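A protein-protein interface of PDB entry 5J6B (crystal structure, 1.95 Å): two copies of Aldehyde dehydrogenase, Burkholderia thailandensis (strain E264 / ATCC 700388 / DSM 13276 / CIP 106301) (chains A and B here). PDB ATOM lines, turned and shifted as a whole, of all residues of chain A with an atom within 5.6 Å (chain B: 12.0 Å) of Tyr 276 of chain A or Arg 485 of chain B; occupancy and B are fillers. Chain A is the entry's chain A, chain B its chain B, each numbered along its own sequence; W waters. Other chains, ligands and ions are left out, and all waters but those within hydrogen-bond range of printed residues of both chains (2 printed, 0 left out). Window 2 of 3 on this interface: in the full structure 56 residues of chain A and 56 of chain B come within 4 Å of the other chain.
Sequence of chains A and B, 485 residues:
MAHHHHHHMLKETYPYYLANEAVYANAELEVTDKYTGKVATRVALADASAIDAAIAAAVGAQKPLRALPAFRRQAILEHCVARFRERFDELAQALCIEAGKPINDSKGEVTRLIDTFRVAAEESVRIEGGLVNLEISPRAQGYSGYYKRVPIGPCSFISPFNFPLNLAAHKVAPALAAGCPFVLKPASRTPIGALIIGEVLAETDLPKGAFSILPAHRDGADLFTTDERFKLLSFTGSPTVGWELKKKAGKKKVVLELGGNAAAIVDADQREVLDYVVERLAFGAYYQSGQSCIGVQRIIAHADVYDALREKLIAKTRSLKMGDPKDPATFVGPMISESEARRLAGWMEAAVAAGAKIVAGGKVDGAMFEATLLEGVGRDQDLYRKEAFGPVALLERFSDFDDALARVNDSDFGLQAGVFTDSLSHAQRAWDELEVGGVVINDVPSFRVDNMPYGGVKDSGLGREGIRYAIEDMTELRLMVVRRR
OH of Tyr 143 of chain B lies within hydrogen-bond range of OD2 of Asp 443 of chain A, 2.4 Å away.
The guanidinium group (NH1) of Arg 483 of chain B lies within salt-bridge range of the side-chain carboxylate (OD2) of Asp 443 of chain A, at 3.8 Å.
The guanidinium group (NH1) of Arg 483 of chain B lies within hydrogen-bond range of the side-chain hydroxyl (OH) of Tyr 276 of chain A (3.1 Å).
Water W1 lies within hydrogen-bond range of the backbone carbonyl oxygen of Arg 483 of chain B (2.6 Å) and the side-chain amide nitrogen of Asn 442 of chain A (2.9 Å).
Water W2 bridges NH1 of Arg 483 of chain B (2.8 Å) and NH1 of Arg 280 of chain A (3.3 Å).
Of chain B, only Arg 485 comes within 4 Å of Val 273 of chain A.
No residue of chain B comes within 4 Å of Val 277 of chain A.
Arg 280 of chain A touches just one residue of chain B: Arg 483.
Asp 443 of chain A touches two residues of chain B.
Printed residues of chain A within 4 Å of Tyr 143 of chain B: Asp 443.
Printed residues of chain A within 4 Å of Arg 483 of chain B: Tyr 276 (3.1 Å), Arg 280 (3.7 Å), Asn 442 (3.6 Å) and Asp 443 (3.8 Å).
Leu 281 of chain A touches none of the printed residues of chain B.
Val 481 of chain B touches none of the printed residues of chain A.
The nearest residue of chain B that does not touch Tyr 276 of chain A is Tyr 143 of chain B (5.1 Å).
The nearest residue of chain A that does not touch Arg 485 of chain B is Asn 442 of chain A (5.4 Å).
The nearest printed residue of chain A that does not touch Tyr 143 of chain B is Arg 280 of chain A (4.02 Å).
The side-chain hydroxyl of Tyr 143 of chain B sits close to the guanidinium group of Arg 483 of chain B.
The backbone carbonyl oxygen of Asn 442 of chain A lies within hydrogen-bond range of the side-chain hydroxyl of Tyr 276 of chain A (2.7 Å).
The side-chain carboxylate (OD1) of Asp 443 of chain A is in salt-bridge range of the guanidinium group (NE) of Arg 280 of chain A (2.6 Å).
No position is printed for both chains.
Among the printed residues, pairs that only touch across the chains: Tyr 276 of chain A with Arg 485 of chain B (3.4 Å), Asn 442 of chain A with Arg 483 of chain B (3.6 Å), Arg 280 of chain A with Arg 483 of chain B (3.7 Å) and Val 273 of chain A with Arg 485 of chain B (3.7 Å).
Of the 14 printed residues of chain B, 3 touch a printed residue of chain A.
Hydrophobic or aromatic side chains of chain B within 4 Å of the printed part of chain A: Tyr 143.
Of the 12 printed residues of chain A, 5 touch a printed residue of chain B.
Printed residues of chain A that touch a printed residue of chain B: Val 273, Tyr 276, Arg 280, Asn 442 and Asp 443.
Hydrophobic or aromatic side chains of chain A within 4 Å of the printed part of chain B: Val 273 and Tyr 276.
Among the printed residues, Asp or Glu carboxylates within 4 Å of a Lys or Arg side-chain nitrogen of the other chain: Asp 443 of chain A with Arg 483 of chain B.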
ATOM      1  N   VAL A 273     -10.394  -0.934  -7.507  1.00  0.00           N
ATOM      2  CA  VAL A 273      -9.802  -0.848  -6.174  1.00  0.00           C
ATOM      3  C   VAL A 273     -10.608   0.069  -5.251  1.00  0.00           C
ATOM      4  O   VAL A 273     -10.075   0.589  -4.277  1.00  0.00           O
ATOM      5  CB  VAL A 273      -8.330  -0.397  -6.251  1.00  0.00           C
ATOM      6  CG1 VAL A 273      -7.466  -1.469  -6.925  1.00  0.00           C
ATOM      7  CG2 VAL A 273      -8.227   0.952  -6.975  1.00  0.00           C
ATOM      8  N   LEU A 274     -11.904   0.255  -5.535  1.00  0.00           N
ATOM      9  CA  LEU A 274     -12.685   1.224  -4.771  1.00  0.00           C
ATOM     10  C   LEU A 274     -12.814   0.837  -3.297  1.00  0.00           C
ATOM     11  O   LEU A 274     -12.885   1.718  -2.434  1.00  0.00           O
ATOM     12  CB  LEU A 274     -14.070   1.410  -5.402  1.00  0.00           C
ATOM     13  CG  LEU A 274     -14.137   2.291  -6.653  1.00  0.00           C
ATOM     14  CD1 LEU A 274     -15.573   2.437  -7.121  1.00  0.00           C
ATOM     15  CD2 LEU A 274     -13.519   3.672  -6.412  1.00  0.00           C
ATOM     16  N   ASP A 275     -12.842  -0.456  -2.975  1.00  0.00           N
ATOM     17  CA  ASP A 275     -12.956  -0.818  -1.561  1.00  0.00           C
ATOM     18  C   ASP A 275     -11.730  -0.364  -0.777  1.00  0.00           C
ATOM     19  O   ASP A 275     -11.848   0.079   0.374  1.00  0.00           O
ATOM     20  CB  ASP A 275     -13.171  -2.321  -1.402  1.00  0.00           C
ATOM     21  CG  ASP A 275     -14.596  -2.724  -1.683  1.00  0.00           C
ATOM     22  OD1 ASP A 275     -15.493  -1.866  -1.559  1.00  0.00           O
ATOM     23  OD2 ASP A 275     -14.821  -3.895  -2.027  1.00  0.00           O
ATOM     24  N   TYR A 276     -10.544  -0.475  -1.380  1.00  0.00           N
ATOM     25  CA  TYR A 276      -9.338   0.033  -0.734  1.00  0.00           C
ATOM     26  C   TYR A 276      -9.381   1.554  -0.614  1.00  0.00           C
ATOM     27  O   TYR A 276      -9.039   2.113   0.438  1.00  0.00           O
ATOM     28  CB  TYR A 276      -8.090  -0.406  -1.504  1.00  0.00           C
ATOM     29  CG  TYR A 276      -6.891   0.460  -1.172  1.00  0.00           C
ATOM     30  CD1 TYR A 276      -6.173   0.254   0.000  1.00  0.00           C
ATOM     31  CD2 TYR A 276      -6.503   1.510  -2.009  1.00  0.00           C
ATOM     32  CE1 TYR A 276      -5.085   1.052   0.329  1.00  0.00           C
ATOM     33  CE2 TYR A 276      -5.408   2.326  -1.680  1.00  0.00           C
ATOM     34  CZ  TYR A 276      -4.714   2.090  -0.508  1.00  0.00           C
ATOM     35  OH  TYR A 276      -3.643   2.888  -0.162  1.00  0.00           O
ATOM     36  N   VAL A 277      -9.790   2.237  -1.682  1.00  0.00           N
ATOM     37  CA  VAL A 277      -9.878   3.696  -1.649  1.00  0.00           C
ATOM     38  C   VAL A 277     -10.835   4.154  -0.553  1.00  0.00           C
ATOM     39  O   VAL A 277     -10.521   5.062   0.230  1.00  0.00           O
ATOM     40  CB  VAL A 277     -10.299   4.226  -3.033  1.00  0.00           C
ATOM     41  CG1 VAL A 277     -10.511   5.746  -2.994  1.00  0.00           C
ATOM     42  CG2 VAL A 277      -9.247   3.853  -4.074  1.00  0.00           C
ATOM     43  N   VAL A 278     -12.002   3.514  -0.458  1.00  0.00           N
ATOM     44  CA  VAL A 278     -12.996   3.900   0.546  1.00  0.00           C
ATOM     45  C   VAL A 278     -12.459   3.670   1.953  1.00  0.00           C
ATOM     46  O   VAL A 278     -12.671   4.489   2.859  1.00  0.00           O
ATOM     47  CB  VAL A 278     -14.315   3.145   0.302  1.00  0.00           C
ATOM     48  CG1 VAL A 278     -15.254   3.261   1.508  1.00  0.00           C
ATOM     49  CG2 VAL A 278     -14.979   3.698  -0.961  1.00  0.00           C
ATOM     50  N   GLU A 279     -11.765   2.552   2.162  1.00  0.00           N
ATOM     51  CA  GLU A 279     -11.182   2.275   3.470  1.00  0.00           C
ATOM     52  C   GLU A 279     -10.203   3.372   3.886  1.00  0.00           C
ATOM     53  O   GLU A 279     -10.204   3.817   5.045  1.00  0.00           O
ATOM     54  CB  GLU A 279     -10.488   0.914   3.431  1.00  0.00           C
ATOM     55  CG  GLU A 279      -9.586   0.670   4.605  1.00  0.00           C
ATOM     56  CD  GLU A 279     -10.377   0.407   5.856  1.00  0.00           C
ATOM     57  OE1 GLU A 279     -11.514  -0.101   5.729  1.00  0.00           O
ATOM     58  OE2 GLU A 279      -9.869   0.714   6.958  1.00  0.00           O
ATOM     59  N   ARG A 280      -9.359   3.824   2.951  1.00  0.00           N
ATOM     60  CA  ARG A 280      -8.378   4.858   3.272  1.00  0.00           C
ATOM     61  C   ARG A 280      -9.041   6.221   3.439  1.00  0.00           C
ATOM     62  O   ARG A 280      -8.645   7.004   4.311  1.00  0.00           O
ATOM     63  CB  ARG A 280      -7.290   4.905   2.191  1.00  0.00           C
ATOM     64  CG  ARG A 280      -6.462   3.618   2.112  1.00  0.00           C
ATOM     65  CD  ARG A 280      -5.942   3.217   3.502  1.00  0.00           C
ATOM     66  NE  ARG A 280      -4.843   4.085   3.912  1.00  0.00           N
ATOM     67  CZ  ARG A 280      -4.349   4.166   5.140  1.00  0.00           C
ATOM     68  NH1 ARG A 280      -4.864   3.434   6.124  1.00  0.00           N
ATOM     69  NH2 ARG A 280      -3.333   4.985   5.381  1.00  0.00           N
ATOM     70  N   LEU A 281     -10.056   6.521   2.626  1.00  0.00           N
ATOM     71  CA  LEU A 281     -10.792   7.768   2.797  1.00  0.00           C
ATOM     72  C   LEU A 281     -11.460   7.819   4.166  1.00  0.00           C
ATOM     73  O   LEU A 281     -11.369   8.822   4.882  1.00  0.00           O
ATOM     74  CB  LEU A 281     -11.845   7.926   1.695  1.00  0.00           C
ATOM     75  CG  LEU A 281     -11.367   8.162   0.262  1.00  0.00           C
ATOM     76  CD1 LEU A 281     -12.573   8.116  -0.691  1.00  0.00           C
ATOM     77  CD2 LEU A 281     -10.627   9.503   0.158  1.00  0.00           C
ATOM     78  N   PHE A 420      -5.477   9.126  -5.773  1.00  0.00           N
ATOM     79  CA  PHE A 420      -5.582   7.711  -6.126  1.00  0.00           C
ATOM     80  C   PHE A 420      -5.661   7.609  -7.650  1.00  0.00           C
ATOM     81  O   PHE A 420      -6.651   8.024  -8.260  1.00  0.00           O
ATOM     82  CB  PHE A 420      -6.800   7.059  -5.466  1.00  0.00           C
ATOM     83  CG  PHE A 420      -6.776   7.077  -3.967  1.00  0.00           C
ATOM     84  CD1 PHE A 420      -6.267   5.995  -3.249  1.00  0.00           C
ATOM     85  CD2 PHE A 420      -7.289   8.165  -3.261  1.00  0.00           C
ATOM     86  CE1 PHE A 420      -6.260   6.002  -1.851  1.00  0.00           C
ATOM     87  CE2 PHE A 420      -7.282   8.181  -1.863  1.00  0.00           C
ATOM     88  CZ  PHE A 420      -6.767   7.097  -1.156  1.00  0.00           C
ATOM     89  N   ASN A 442      -1.839   7.254  -4.211  1.00  0.00           N
ATOM     90  CA  ASN A 442      -2.489   5.982  -3.894  1.00  0.00           C
ATOM     91  C   ASN A 442      -2.589   5.724  -2.399  1.00  0.00           C
ATOM     92  O   ASN A 442      -2.664   4.577  -1.960  1.00  0.00           O
ATOM     93  CB  ASN A 442      -1.816   4.824  -4.625  1.00  0.00           C
ATOM     94  CG  ASN A 442      -2.199   4.824  -6.092  1.00  0.00           C
ATOM     95  OD1 ASN A 442      -3.370   5.028  -6.412  1.00  0.00           O
ATOM     96  ND2 ASN A 442      -1.237   4.630  -6.976  1.00  0.00           N
ATOM     97  N   ASP A 443      -2.610   6.805  -1.628  1.00  0.00           N
ATOM     98  CA  ASP A 443      -3.085   6.815  -0.253  1.00  0.00           C
ATOM     99  C   ASP A 443      -3.580   8.230   0.028  1.00  0.00           C
ATOM    100  O   ASP A 443      -3.370   9.151  -0.768  1.00  0.00           O
ATOM    101  CB  ASP A 443      -1.993   6.373   0.727  1.00  0.00           C
ATOM    102  CG  ASP A 443      -2.558   5.884   2.070  1.00  0.00           C
ATOM    103  OD1 ASP A 443      -3.801   5.823   2.248  1.00  0.00           O
ATOM    104  OD2 ASP A 443      -1.737   5.546   2.947  1.00  0.00           O
ATOM    105  N   GLU B 135      10.424   2.957   4.126  1.00  0.00           N
ATOM    106  CA  GLU B 135      10.019   1.650   4.639  1.00  0.00           C
ATOM    107  C   GLU B 135      10.774   1.362   5.940  1.00  0.00           C
ATOM    108  O   GLU B 135      11.627   0.479   6.029  1.00  0.00           O
ATOM    109  CB  GLU B 135      10.265   0.568   3.595  1.00  0.00           C
ATOM    110  CG  GLU B 135       9.285   0.565   2.446  1.00  0.00           C
ATOM    111  CD  GLU B 135       9.443  -0.671   1.561  1.00  0.00           C
ATOM    112  OE1 GLU B 135      10.501  -0.805   0.913  1.00  0.00           O
ATOM    113  OE2 GLU B 135       8.524  -1.515   1.526  1.00  0.00           O
ATOM    114  N   PRO B 138       6.601  -1.554   9.697  1.00  0.00           N
ATOM    115  CA  PRO B 138       5.634  -2.349   8.921  1.00  0.00           C
ATOM    116  C   PRO B 138       4.492  -1.532   8.359  1.00  0.00           C
ATOM    117  O   PRO B 138       4.037  -1.804   7.239  1.00  0.00           O
ATOM    118  CB  PRO B 138       5.154  -3.393   9.945  1.00  0.00           C
ATOM    119  CG  PRO B 138       6.349  -3.569  10.864  1.00  0.00           C
ATOM    120  CD  PRO B 138       6.904  -2.176  11.006  1.00  0.00           C
ATOM    121  N   ARG B 139       4.023  -0.534   9.115  1.00  0.00           N
ATOM    122  CA  ARG B 139       3.005   0.401   8.647  1.00  0.00           C
ATOM    123  C   ARG B 139       3.389   1.057   7.317  1.00  0.00           C
ATOM    124  O   ARG B 139       2.518   1.356   6.492  1.00  0.00           O
ATOM    125  CB  ARG B 139       2.799   1.478   9.723  1.00  0.00           C
ATOM    126  CG  ARG B 139       1.604   2.373   9.559  1.00  0.00           C
ATOM    127  CD  ARG B 139       1.479   3.297  10.767  1.00  0.00           C
ATOM    128  NE  ARG B 139       2.623   4.198  10.875  1.00  0.00           N
ATOM    129  CZ  ARG B 139       2.684   5.380  10.273  1.00  0.00           C
ATOM    130  NH1 ARG B 139       1.662   5.781   9.531  1.00  0.00           N
ATOM    131  NH2 ARG B 139       3.757   6.155  10.403  1.00  0.00           N
ATOM    132  N   ALA B 140       4.676   1.309   7.098  1.00  0.00           N
ATOM    133  CA  ALA B 140       5.127   2.023   5.911  1.00  0.00           C
ATOM    134  C   ALA B 140       5.685   1.094   4.832  1.00  0.00           C
ATOM    135  O   ALA B 140       6.398   1.556   3.943  1.00  0.00           O
ATOM    136  CB  ALA B 140       6.163   3.083   6.299  1.00  0.00           C
ATOM    137  N   GLN B 141       5.377  -0.200   4.882  1.00  0.00           N
ATOM    138  CA  GLN B 141       5.809  -1.085   3.807  1.00  0.00           C
ATOM    139  C   GLN B 141       5.121  -0.694   2.500  1.00  0.00           C
ATOM    140  O   GLN B 141       3.916  -0.437   2.470  1.00  0.00           O
ATOM    141  CB  GLN B 141       5.501  -2.545   4.151  1.00  0.00           C
ATOM    142  CG  GLN B 141       6.031  -3.523   3.119  1.00  0.00           C
ATOM    143  CD  GLN B 141       5.907  -4.978   3.555  1.00  0.00           C
ATOM    144  OE1 GLN B 141       5.663  -5.271   4.726  1.00  0.00           O
ATOM    145  NE2 GLN B 141       6.067  -5.893   2.607  1.00  0.00           N
ATOM    146  N   GLY B 142       5.896  -0.645   1.412  1.00  0.00           N
ATOM    147  CA  GLY B 142       5.363  -0.294   0.107  1.00  0.00           C
ATOM    148  C   GLY B 142       5.349   1.188  -0.229  1.00  0.00           C
ATOM    149  O   GLY B 142       4.966   1.551  -1.350  1.00  0.00           O
ATOM    150  N   TYR B 143       5.745   2.059   0.688  1.00  0.00           N
ATOM    151  CA  TYR B 143       5.799   3.488   0.403  1.00  0.00           C
ATOM    152  C   TYR B 143       7.218   3.882  -0.007  1.00  0.00           C
ATOM    153  O   TYR B 143       8.196   3.359   0.534  1.00  0.00           O
ATOM    154  CB  TYR B 143       5.379   4.308   1.623  1.00  0.00           C
ATOM    155  CG  TYR B 143       3.924   4.174   2.059  1.00  0.00           C
ATOM    156  CD1 TYR B 143       3.486   3.050   2.754  1.00  0.00           C
ATOM    157  CD2 TYR B 143       3.002   5.199   1.818  1.00  0.00           C
ATOM    158  CE1 TYR B 143       2.160   2.933   3.190  1.00  0.00           C
ATOM    159  CE2 TYR B 143       1.673   5.092   2.245  1.00  0.00           C
ATOM    160  CZ  TYR B 143       1.264   3.958   2.940  1.00  0.00           C
ATOM    161  OH  TYR B 143      -0.045   3.831   3.374  1.00  0.00           O
ATOM    162  N   SER B 144       7.329   4.818  -0.945  1.00  0.00           N
ATOM    163  CA  SER B 144       8.620   5.387  -1.310  1.00  0.00           C
ATOM    164  C   SER B 144       8.489   6.903  -1.379  1.00  0.00           C
ATOM    165  O   SER B 144       7.396   7.433  -1.592  1.00  0.00           O
ATOM    166  CB  SER B 144       9.135   4.816  -2.649  1.00  0.00           C
ATOM    167  OG  SER B 144       8.115   4.830  -3.630  1.00  0.00           O
ATOM    168  N   TYR B 146      10.003  10.769  -2.779  1.00  0.00           N
ATOM    169  CA  TYR B 146      10.722  11.572  -3.756  1.00  0.00           C
ATOM    170  C   TYR B 146      10.481  13.030  -3.413  1.00  0.00           C
ATOM    171  O   TYR B 146       9.351  13.410  -3.096  1.00  0.00           O
ATOM    172  CB  TYR B 146      10.207  11.320  -5.184  1.00  0.00           C
ATOM    173  CG  TYR B 146      10.075   9.859  -5.535  1.00  0.00           C
ATOM    174  CD1 TYR B 146       8.970   9.121  -5.119  1.00  0.00           C
ATOM    175  CD2 TYR B 146      11.054   9.213  -6.279  1.00  0.00           C
ATOM    176  CE1 TYR B 146       8.850   7.785  -5.422  1.00  0.00           C
ATOM    177  CE2 TYR B 146      10.942   7.869  -6.589  1.00  0.00           C
ATOM    178  CZ  TYR B 146       9.838   7.162  -6.162  1.00  0.00           C
ATOM    179  OH  TYR B 146       9.719   5.825  -6.470  1.00  0.00           O
ATOM    180  N   VAL B 481       4.976  11.119  -1.961  1.00  0.00           N
ATOM    181  CA  VAL B 481       4.933   9.797  -1.351  1.00  0.00           C
ATOM    182  C   VAL B 481       4.121   8.903  -2.273  1.00  0.00           C
ATOM    183  O   VAL B 481       2.981   9.228  -2.611  1.00  0.00           O
ATOM    184  CB  VAL B 481       4.307   9.859   0.057  1.00  0.00           C
ATOM    185  CG1 VAL B 481       4.125   8.426   0.667  1.00  0.00           C
ATOM    186  CG2 VAL B 481       5.156  10.743   0.961  1.00  0.00           C
ATOM    187  N   VAL B 482       4.694   7.773  -2.675  1.00  0.00           N
ATOM    188  CA  VAL B 482       4.019   6.833  -3.557  1.00  0.00           C
ATOM    189  C   VAL B 482       3.838   5.521  -2.811  1.00  0.00           C
ATOM    190  O   VAL B 482       4.818   4.957  -2.317  1.00  0.00           O
ATOM    191  CB  VAL B 482       4.813   6.612  -4.853  1.00  0.00           C
ATOM    192  CG1 VAL B 482       4.034   5.689  -5.772  1.00  0.00           C
ATOM    193  CG2 VAL B 482       5.078   7.947  -5.535  1.00  0.00           C
ATOM    194  N   ARG B 483       2.591   5.036  -2.742  1.00  0.00           N
ATOM    195  CA  ARG B 483       2.278   3.755  -2.113  1.00  0.00           C
ATOM    196  C   ARG B 483       2.058   2.700  -3.190  1.00  0.00           C
ATOM    197  O   ARG B 483       1.217   2.875  -4.080  1.00  0.00           O
ATOM    198  CB  ARG B 483       1.041   3.829  -1.211  1.00  0.00           C
ATOM    199  CG  ARG B 483       0.885   2.533  -0.408  1.00  0.00           C
ATOM    200  CD  ARG B 483      -0.440   2.393   0.320  1.00  0.00           C
ATOM    201  NE  ARG B 483      -0.321   1.368   1.350  1.00  0.00           N
ATOM    202  CZ  ARG B 483      -1.205   1.154   2.323  1.00  0.00           C
ATOM    203  NH1 ARG B 483      -2.327   1.869   2.405  1.00  0.00           N
ATOM    204  NH2 ARG B 483      -0.962   0.212   3.217  1.00  0.00           N
ATOM    205  N   ARG B 484       2.817   1.618  -3.116  1.00  0.00           N
ATOM    206  CA  ARG B 484       2.573   0.440  -3.926  1.00  0.00           C
ATOM    207  C   ARG B 484       2.015  -0.656  -3.026  1.00  0.00           C
ATOM    208  O   ARG B 484       2.354  -0.738  -1.836  1.00  0.00           O
ATOM    209  CB  ARG B 484       3.858  -0.016  -4.622  1.00  0.00           C
ATOM    210  CG  ARG B 484       4.512   1.096  -5.442  1.00  0.00           C
ATOM    211  CD  ARG B 484       5.810   0.630  -6.054  1.00  0.00           C
ATOM    212  NE  ARG B 484       5.615  -0.564  -6.872  1.00  0.00           N
ATOM    213  CZ  ARG B 484       6.610  -1.339  -7.289  1.00  0.00           C
ATOM    214  NH1 ARG B 484       7.859  -1.042  -6.952  1.00  0.00           N
ATOM    215  NH2 ARG B 484       6.356  -2.410  -8.032  1.00  0.00           N
ATOM    216  N   ARG B 485       1.126  -1.467  -3.586  1.00  0.00           N
ATOM    217  CA  ARG B 485       0.439  -2.497  -2.801  1.00  0.00           C
ATOM    218  C   ARG B 485       0.540  -3.877  -3.450  1.00  0.00           C
ATOM    219  O   ARG B 485       0.699  -3.996  -4.665  1.00  0.00           O
ATOM    220  CB  ARG B 485      -1.037  -2.136  -2.604  1.00  0.00           C
ATOM    221  CG  ARG B 485      -1.300  -0.873  -1.803  1.00  0.00           C
ATOM    222  CD  ARG B 485      -2.761  -0.832  -1.365  1.00  0.00           C
ATOM    223  NE  ARG B 485      -3.652  -0.760  -2.514  1.00  0.00           N
ATOM    224  CZ  ARG B 485      -4.637  -1.617  -2.773  1.00  0.00           C
ATOM    225  NH1 ARG B 485      -5.378  -1.454  -3.862  1.00  0.00           N
ATOM    226  NH2 ARG B 485      -4.898  -2.624  -1.949  1.00  0.00           N
ATOM    227  OXT ARG B 485       0.445  -4.904  -2.770  1.00  0.00           O
HETATM  228  O   HOH W   1       1.438   3.574  -6.566  1.00  0.00           O
HETATM  229  O   HOH W   2      -3.396   0.772   4.757  1.00  0.00           O
